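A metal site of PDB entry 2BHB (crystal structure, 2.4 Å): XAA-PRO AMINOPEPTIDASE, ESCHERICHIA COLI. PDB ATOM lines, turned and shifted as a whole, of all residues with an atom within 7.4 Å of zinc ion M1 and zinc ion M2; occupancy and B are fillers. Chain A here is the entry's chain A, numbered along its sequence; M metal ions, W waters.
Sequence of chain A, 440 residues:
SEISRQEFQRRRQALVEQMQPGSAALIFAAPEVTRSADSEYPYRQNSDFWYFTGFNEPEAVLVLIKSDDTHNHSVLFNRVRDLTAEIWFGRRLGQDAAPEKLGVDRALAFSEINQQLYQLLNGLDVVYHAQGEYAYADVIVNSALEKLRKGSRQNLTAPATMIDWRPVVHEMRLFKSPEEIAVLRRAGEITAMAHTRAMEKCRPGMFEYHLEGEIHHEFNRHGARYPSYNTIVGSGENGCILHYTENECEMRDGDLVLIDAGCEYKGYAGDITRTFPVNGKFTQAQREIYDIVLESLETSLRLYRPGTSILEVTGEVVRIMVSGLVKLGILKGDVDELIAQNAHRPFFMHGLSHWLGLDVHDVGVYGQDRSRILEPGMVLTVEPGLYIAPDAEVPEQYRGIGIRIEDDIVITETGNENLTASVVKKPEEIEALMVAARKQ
The backbone carbonyl oxygen (O) of Val 360 lies close to a ring nitrogen (ND1) of His 354, at 2.9 Å. The side-chain hydroxyl (OH) of Tyr 229 sits close to the side-chain carboxylate (OD1) of Asp 260, at 2.7 Å. The side-chain hydroxyl of Tyr 229 sits close to the backbone NH of Ala 261, at 3.0 Å. OE1 of Glu 383 lies within salt-bridge range of NE of Arg 404 (3.9 Å). N of Thr 381 lies within hydrogen-bond range of O of His 354, 3.0 Å away. OD2 of Asp 260 lies close to OG1 of Thr 273 (3.1 Å). N of Glu 406 sits at hydrogen-bond distance from O of Thr 273, 3.0 Å away. N of Asp 271 lies within hydrogen-bond range of OD2 of Asp 408 (2.9 Å).
Residues that only touch zinc ion M1: Thr 381 (3.6 Å). Within 4 Å of zinc ion M1: Asp 271, His 354, Thr 381, Glu 383 and Glu 406. The nearest printed residue that does not touch zinc ion M1 is His 361 (4.6 Å).
Zinc ion M2 is bound by water W1 (1.9 Å), OD1 of Asp 260 (2.0 Å), OE1 of Glu 406 (2.1 Å), OD1 of Asp 271 (2.1 Å) and OD2 of Asp 260 (2.6 Å).
Zinc ion M1 is bound by water W1, a ring nitrogen (NE2) of His 354, the side-chain carboxylate (OE2) of Glu 406, the side-chain carboxylate (OD2) of Asp 271 and the side-chain carboxylate (OE2) of Glu 383. Zinc ion M1 has five donor atoms within binding distance.
Tyr 229 touches zinc ion M2 (OH to ZN, 3.7 Å). Thr 273 touches zinc ion M2 (OG1 to ZN, 3.6 Å). Within 4 Å of zinc ion M2: Tyr 229, Asp 260, Asp 271, Thr 273 and Glu 406.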
ATOM      1  N   TYR A 229     -12.865  31.000 -10.235  1.00  0.00           N
ATOM      2  CA  TYR A 229     -11.821  30.952 -11.254  1.00  0.00           C
ATOM      3  C   TYR A 229     -12.074  32.070 -12.264  1.00  0.00           C
ATOM      4  O   TYR A 229     -13.166  32.622 -12.318  1.00  0.00           O
ATOM      5  CB  TYR A 229     -11.777  29.568 -11.941  1.00  0.00           C
ATOM      6  CG  TYR A 229     -13.102  29.159 -12.535  1.00  0.00           C
ATOM      7  CD1 TYR A 229     -14.092  28.611 -11.738  1.00  0.00           C
ATOM      8  CD2 TYR A 229     -13.379  29.359 -13.886  1.00  0.00           C
ATOM      9  CE1 TYR A 229     -15.326  28.266 -12.266  1.00  0.00           C
ATOM     10  CE2 TYR A 229     -14.617  28.993 -14.427  1.00  0.00           C
ATOM     11  CZ  TYR A 229     -15.575  28.453 -13.596  1.00  0.00           C
ATOM     12  OH  TYR A 229     -16.813  28.097 -14.097  1.00  0.00           O
ATOM     13  N   ILE A 232     -14.514  32.620 -18.382  1.00  0.00           N
ATOM     14  CA  ILE A 232     -14.247  32.363 -19.791  1.00  0.00           C
ATOM     15  C   ILE A 232     -15.466  32.777 -20.613  1.00  0.00           C
ATOM     16  O   ILE A 232     -16.545  32.247 -20.402  1.00  0.00           O
ATOM     17  CB  ILE A 232     -13.939  30.855 -20.013  1.00  0.00           C
ATOM     18  CG1 ILE A 232     -12.577  30.493 -19.377  1.00  0.00           C
ATOM     19  CG2 ILE A 232     -13.946  30.473 -21.505  1.00  0.00           C
ATOM     20  CD1 ILE A 232     -12.507  29.086 -18.865  1.00  0.00           C
ATOM     21  N   ILE A 259     -19.583  30.277 -22.350  1.00  0.00           N
ATOM     22  CA  ILE A 259     -19.311  30.903 -21.056  1.00  0.00           C
ATOM     23  C   ILE A 259     -19.060  29.828 -20.012  1.00  0.00           C
ATOM     24  O   ILE A 259     -19.944  29.019 -19.725  1.00  0.00           O
ATOM     25  CB  ILE A 259     -20.475  31.800 -20.606  1.00  0.00           C
ATOM     26  CG1 ILE A 259     -20.796  32.815 -21.704  1.00  0.00           C
ATOM     27  CG2 ILE A 259     -20.132  32.477 -19.276  1.00  0.00           C
ATOM     28  CD1 ILE A 259     -21.777  33.907 -21.286  1.00  0.00           C
ATOM     29  N   ASP A 260     -17.841  29.806 -19.469  1.00  0.00           N
ATOM     30  CA  ASP A 260     -17.475  28.977 -18.319  1.00  0.00           C
ATOM     31  C   ASP A 260     -17.201  29.919 -17.138  1.00  0.00           C
ATOM     32  O   ASP A 260     -16.220  30.666 -17.132  1.00  0.00           O
ATOM     33  CB  ASP A 260     -16.245  28.116 -18.623  1.00  0.00           C
ATOM     34  CG  ASP A 260     -16.120  26.888 -17.690  1.00  0.00           C
ATOM     35  OD1 ASP A 260     -16.637  26.874 -16.544  1.00  0.00           O
ATOM     36  OD2 ASP A 260     -15.482  25.913 -18.122  1.00  0.00           O
ATOM     37  N   ALA A 261     -18.103  29.888 -16.166  1.00  0.00           N
ATOM     38  CA  ALA A 261     -18.050  30.829 -15.061  1.00  0.00           C
ATOM     39  C   ALA A 261     -18.709  30.233 -13.821  1.00  0.00           C
ATOM     40  O   ALA A 261     -19.685  29.480 -13.902  1.00  0.00           O
ATOM     41  CB  ALA A 261     -18.725  32.144 -15.441  1.00  0.00           C
ATOM     42  N   GLY A 262     -18.149  30.584 -12.661  1.00  0.00           N
ATOM     43  CA  GLY A 262     -18.552  30.025 -11.394  1.00  0.00           C
ATOM     44  C   GLY A 262     -18.225  30.980 -10.272  1.00  0.00           C
ATOM     45  O   GLY A 262     -17.180  31.631 -10.290  1.00  0.00           O
ATOM     46  N   GLY A 270     -19.049  27.238  -7.482  1.00  0.00           N
ATOM     47  CA  GLY A 270     -19.935  26.890  -8.570  1.00  0.00           C
ATOM     48  C   GLY A 270     -19.078  26.791  -9.818  1.00  0.00           C
ATOM     49  O   GLY A 270     -17.990  27.343  -9.869  1.00  0.00           O
ATOM     50  N   ASP A 271     -19.567  26.081 -10.824  1.00  0.00           N
ATOM     51  CA  ASP A 271     -18.803  25.858 -12.048  1.00  0.00           C
ATOM     52  C   ASP A 271     -19.738  25.429 -13.177  1.00  0.00           C
ATOM     53  O   ASP A 271     -20.047  24.232 -13.324  1.00  0.00           O
ATOM     54  CB  ASP A 271     -17.716  24.814 -11.799  1.00  0.00           C
ATOM     55  CG  ASP A 271     -16.844  24.598 -13.005  1.00  0.00           C
ATOM     56  OD1 ASP A 271     -17.002  25.341 -13.988  1.00  0.00           O
ATOM     57  OD2 ASP A 271     -15.999  23.688 -12.964  1.00  0.00           O
ATOM     58  N   ILE A 272     -20.209  26.388 -13.962  1.00  0.00           N
ATOM     59  CA  ILE A 272     -21.149  26.106 -15.045  1.00  0.00           C
ATOM     60  C   ILE A 272     -20.566  26.557 -16.396  1.00  0.00           C
ATOM     61  O   ILE A 272     -19.874  27.573 -16.482  1.00  0.00           O
ATOM     62  CB  ILE A 272     -22.518  26.804 -14.792  1.00  0.00           C
ATOM     63  CG1 ILE A 272     -23.215  26.213 -13.580  1.00  0.00           C
ATOM     64  CG2 ILE A 272     -23.452  26.696 -16.025  1.00  0.00           C
ATOM     65  CD1 ILE A 272     -24.519  26.905 -13.238  1.00  0.00           C
ATOM     66  N   THR A 273     -20.852  25.776 -17.437  1.00  0.00           N
ATOM     67  CA  THR A 273     -20.619  26.213 -18.813  1.00  0.00           C
ATOM     68  C   THR A 273     -21.925  26.149 -19.568  1.00  0.00           C
ATOM     69  O   THR A 273     -22.635  25.140 -19.522  1.00  0.00           O
ATOM     70  CB  THR A 273     -19.577  25.376 -19.602  1.00  0.00           C
ATOM     71  OG1 THR A 273     -18.407  25.148 -18.805  1.00  0.00           O
ATOM     72  CG2 THR A 273     -19.151  26.138 -20.873  1.00  0.00           C
ATOM     73  N   LEU A 352     -14.077  14.577 -18.726  1.00  0.00           N
ATOM     74  CA  LEU A 352     -15.510  14.819 -18.620  1.00  0.00           C
ATOM     75  C   LEU A 352     -15.898  15.453 -17.276  1.00  0.00           C
ATOM     76  O   LEU A 352     -16.895  16.174 -17.172  1.00  0.00           O
ATOM     77  CB  LEU A 352     -16.253  13.493 -18.760  1.00  0.00           C
ATOM     78  CG  LEU A 352     -17.784  13.530 -18.770  1.00  0.00           C
ATOM     79  CD1 LEU A 352     -18.279  14.321 -19.957  1.00  0.00           C
ATOM     80  CD2 LEU A 352     -18.332  12.116 -18.776  1.00  0.00           C
ATOM     81  N   SER A 353     -15.128  15.158 -16.240  1.00  0.00           N
ATOM     82  CA  SER A 353     -15.545  15.435 -14.877  1.00  0.00           C
ATOM     83  C   SER A 353     -14.361  15.700 -13.980  1.00  0.00           C
ATOM     84  O   SER A 353     -13.386  14.969 -14.023  1.00  0.00           O
ATOM     85  CB  SER A 353     -16.339  14.247 -14.311  1.00  0.00           C
ATOM     86  OG  SER A 353     -17.573  14.070 -14.975  1.00  0.00           O
ATOM     87  N   HIS A 354     -14.449  16.744 -13.148  1.00  0.00           N
ATOM     88  CA  HIS A 354     -13.511  16.916 -12.063  1.00  0.00           C
ATOM     89  C   HIS A 354     -14.257  17.057 -10.737  1.00  0.00           C
ATOM     90  O   HIS A 354     -15.423  17.452 -10.712  1.00  0.00           O
ATOM     91  CB  HIS A 354     -12.554  18.100 -12.306  1.00  0.00           C
ATOM     92  CG  HIS A 354     -13.244  19.414 -12.527  1.00  0.00           C
ATOM     93  ND1 HIS A 354     -13.723  20.183 -11.480  1.00  0.00           N
ATOM     94  CD2 HIS A 354     -13.523  20.095 -13.658  1.00  0.00           C
ATOM     95  CE1 HIS A 354     -14.278  21.281 -11.983  1.00  0.00           C
ATOM     96  NE2 HIS A 354     -14.160  21.254 -13.291  1.00  0.00           N
ATOM     97  N   TRP A 355     -13.582  16.714  -9.649  1.00  0.00           N
ATOM     98  CA  TRP A 355     -14.099  16.939  -8.302  1.00  0.00           C
ATOM     99  C   TRP A 355     -14.346  18.445  -8.109  1.00  0.00           C
ATOM    100  O   TRP A 355     -13.610  19.275  -8.636  1.00  0.00           O
ATOM    101  CB  TRP A 355     -13.124  16.473  -7.223  1.00  0.00           C
ATOM    102  CG  TRP A 355     -12.621  15.064  -7.287  1.00  0.00           C
ATOM    103  CD1 TRP A 355     -11.323  14.668  -7.174  1.00  0.00           C
ATOM    104  CD2 TRP A 355     -13.397  13.858  -7.426  1.00  0.00           C
ATOM    105  NE1 TRP A 355     -11.233  13.304  -7.242  1.00  0.00           N
ATOM    106  CE2 TRP A 355     -12.492  12.779  -7.403  1.00  0.00           C
ATOM    107  CE3 TRP A 355     -14.762  13.600  -7.581  1.00  0.00           C
ATOM    108  CZ2 TRP A 355     -12.911  11.452  -7.524  1.00  0.00           C
ATOM    109  CZ3 TRP A 355     -15.180  12.273  -7.680  1.00  0.00           C
ATOM    110  CH2 TRP A 355     -14.250  11.213  -7.664  1.00  0.00           C
ATOM    111  N   LEU A 356     -15.348  18.788  -7.312  1.00  0.00           N
ATOM    112  CA  LEU A 356     -15.706  20.173  -7.075  1.00  0.00           C
ATOM    113  C   LEU A 356     -15.886  20.426  -5.565  1.00  0.00           C
ATOM    114  O   LEU A 356     -16.480  19.615  -4.852  1.00  0.00           O
ATOM    115  CB  LEU A 356     -16.986  20.505  -7.847  1.00  0.00           C
ATOM    116  CG  LEU A 356     -17.560  21.917  -7.746  1.00  0.00           C
ATOM    117  CD1 LEU A 356     -16.701  22.933  -8.488  1.00  0.00           C
ATOM    118  CD2 LEU A 356     -18.997  21.926  -8.279  1.00  0.00           C
ATOM    119  N   VAL A 360     -12.257  24.746  -7.332  1.00  0.00           N
ATOM    120  CA  VAL A 360     -13.081  24.390  -8.479  1.00  0.00           C
ATOM    121  C   VAL A 360     -12.607  23.051  -9.083  1.00  0.00           C
ATOM    122  O   VAL A 360     -13.432  22.181  -9.351  1.00  0.00           O
ATOM    123  CB  VAL A 360     -13.181  25.543  -9.540  1.00  0.00           C
ATOM    124  CG1 VAL A 360     -11.810  25.898 -10.120  1.00  0.00           C
ATOM    125  CG2 VAL A 360     -14.136  25.146 -10.642  1.00  0.00           C
ATOM    126  N   HIS A 361     -11.308  22.891  -9.268  1.00  0.00           N
ATOM    127  CA  HIS A 361     -10.704  21.584  -9.547  1.00  0.00           C
ATOM    128  C   HIS A 361     -10.257  21.027  -8.217  1.00  0.00           C
ATOM    129  O   HIS A 361      -9.116  21.250  -7.768  1.00  0.00           O
ATOM    130  CB  HIS A 361      -9.539  21.681 -10.531  1.00  0.00           C
ATOM    131  CG  HIS A 361      -9.938  22.121 -11.908  1.00  0.00           C
ATOM    132  ND1 HIS A 361      -9.028  22.555 -12.845  1.00  0.00           N
ATOM    133  CD2 HIS A 361     -11.154  22.247 -12.484  1.00  0.00           C
ATOM    134  CE1 HIS A 361      -9.665  22.907 -13.945  1.00  0.00           C
ATOM    135  NE2 HIS A 361     -10.955  22.718 -13.755  1.00  0.00           N
ATOM    136  N   LEU A 380     -19.002  16.574  -8.228  1.00  0.00           N
ATOM    137  CA  LEU A 380     -18.250  16.648  -9.463  1.00  0.00           C
ATOM    138  C   LEU A 380     -18.987  17.357 -10.594  1.00  0.00           C
ATOM    139  O   LEU A 380     -20.207  17.585 -10.542  1.00  0.00           O
ATOM    140  CB  LEU A 380     -17.833  15.244  -9.924  1.00  0.00           C
ATOM    141  CG  LEU A 380     -18.917  14.193 -10.231  1.00  0.00           C
ATOM    142  CD1 LEU A 380     -18.349  13.150 -11.158  1.00  0.00           C
ATOM    143  CD2 LEU A 380     -19.461  13.549  -8.966  1.00  0.00           C
ATOM    144  N   THR A 381     -18.221  17.722 -11.610  1.00  0.00           N
ATOM    145  CA  THR A 381     -18.750  18.344 -12.788  1.00  0.00           C
ATOM    146  C   THR A 381     -18.987  17.294 -13.885  1.00  0.00           C
ATOM    147  O   THR A 381     -18.437  16.195 -13.849  1.00  0.00           O
ATOM    148  CB  THR A 381     -17.810  19.434 -13.312  1.00  0.00           C
ATOM    149  OG1 THR A 381     -16.624  18.831 -13.861  1.00  0.00           O
ATOM    150  CG2 THR A 381     -17.439  20.391 -12.176  1.00  0.00           C
ATOM    151  N   VAL A 382     -19.850  17.663 -14.833  1.00  0.00           N
ATOM    152  CA  VAL A 382     -20.089  16.885 -16.031  1.00  0.00           C
ATOM    153  C   VAL A 382     -20.020  17.913 -17.135  1.00  0.00           C
ATOM    154  O   VAL A 382     -20.886  18.776 -17.221  1.00  0.00           O
ATOM    155  CB  VAL A 382     -21.481  16.193 -16.000  1.00  0.00           C
ATOM    156  CG1 VAL A 382     -21.591  15.141 -17.108  1.00  0.00           C
ATOM    157  CG2 VAL A 382     -21.744  15.540 -14.637  1.00  0.00           C
ATOM    158  N   GLU A 383     -18.971  17.848 -17.951  1.00  0.00           N
ATOM    159  CA  GLU A 383     -18.701  18.891 -18.920  1.00  0.00           C
ATOM    160  C   GLU A 383     -18.144  18.385 -20.249  1.00  0.00           C
ATOM    161  O   GLU A 383     -17.008  18.713 -20.619  1.00  0.00           O
ATOM    162  CB  GLU A 383     -17.754  19.938 -18.304  1.00  0.00           C
ATOM    163  CG  GLU A 383     -16.426  19.422 -17.805  1.00  0.00           C
ATOM    164  CD  GLU A 383     -15.665  20.486 -17.067  1.00  0.00           C
ATOM    165  OE1 GLU A 383     -15.279  21.509 -17.707  1.00  0.00           O
ATOM    166  OE2 GLU A 383     -15.475  20.314 -15.841  1.00  0.00           O
ATOM    167  N   ARG A 404     -19.163  23.678 -25.098  1.00  0.00           N
ATOM    168  CA  ARG A 404     -19.111  22.923 -23.845  1.00  0.00           C
ATOM    169  C   ARG A 404     -20.397  23.209 -23.089  1.00  0.00           C
ATOM    170  O   ARG A 404     -20.910  24.325 -23.120  1.00  0.00           O
ATOM    171  CB  ARG A 404     -17.868  23.299 -23.013  1.00  0.00           C
ATOM    172  CG  ARG A 404     -17.750  22.599 -21.647  1.00  0.00           C
ATOM    173  CD  ARG A 404     -16.330  22.656 -21.049  1.00  0.00           C
ATOM    174  NE  ARG A 404     -15.816  23.996 -20.698  1.00  0.00           N
ATOM    175  CZ  ARG A 404     -14.960  24.731 -21.414  1.00  0.00           C
ATOM    176  NH1 ARG A 404     -14.488  24.327 -22.590  1.00  0.00           N
ATOM    177  NH2 ARG A 404     -14.568  25.905 -20.962  1.00  0.00           N
ATOM    178  N   GLU A 406     -21.911  22.290 -19.178  1.00  0.00           N
ATOM    179  CA  GLU A 406     -21.436  21.789 -17.899  1.00  0.00           C
ATOM    180  C   GLU A 406     -22.386  22.032 -16.737  1.00  0.00           C
ATOM    181  O   GLU A 406     -22.853  23.149 -16.525  1.00  0.00           O
ATOM    182  CB  GLU A 406     -20.079  22.416 -17.567  1.00  0.00           C
ATOM    183  CG  GLU A 406     -19.651  22.241 -16.114  1.00  0.00           C
ATOM    184  CD  GLU A 406     -18.287  22.797 -15.869  1.00  0.00           C
ATOM    185  OE1 GLU A 406     -17.931  23.809 -16.528  1.00  0.00           O
ATOM    186  OE2 GLU A 406     -17.580  22.241 -15.005  1.00  0.00           O
ATOM    187  N   ASP A 407     -22.647  20.958 -16.001  1.00  0.00           N
ATOM    188  CA  ASP A 407     -23.462  20.985 -14.802  1.00  0.00           C
ATOM    189  C   ASP A 407     -22.614  20.455 -13.632  1.00  0.00           C
ATOM    190  O   ASP A 407     -21.627  19.738 -13.830  1.00  0.00           O
ATOM    191  CB  ASP A 407     -24.728  20.114 -15.005  1.00  0.00           C
ATOM    192  CG  ASP A 407     -25.920  20.906 -15.595  1.00  0.00           C
ATOM    193  OD1 ASP A 407     -25.946  22.155 -15.517  1.00  0.00           O
ATOM    194  OD2 ASP A 407     -26.866  20.270 -16.113  1.00  0.00           O
ATOM    195  N   ASP A 408     -23.001  20.843 -12.418  1.00  0.00           N
ATOM    196  CA  ASP A 408     -22.353  20.385 -11.169  1.00  0.00           C
ATOM    197  C   ASP A 408     -23.302  19.441 -10.428  1.00  0.00           C
ATOM    198  O   ASP A 408     -24.484  19.749 -10.244  1.00  0.00           O
ATOM    199  CB  ASP A 408     -22.036  21.579 -10.244  1.00  0.00           C
ATOM    200  CG  ASP A 408     -21.196  22.637 -10.919  1.00  0.00           C
ATOM    201  OD1 ASP A 408     -20.375  22.292 -11.822  1.00  0.00           O
ATOM    202  OD2 ASP A 408     -21.347  23.817 -10.531  1.00  0.00           O
HETATM  203 ZN    ZN M   1     -15.475  22.306 -14.577  1.00  0.00          ZN
HETATM  204 ZN    ZN M   2     -16.334  24.950 -15.905  1.00  0.00          ZN
HETATM  205  O   HOH W   1     -14.848  23.758 -15.928  1.00  0.00           O
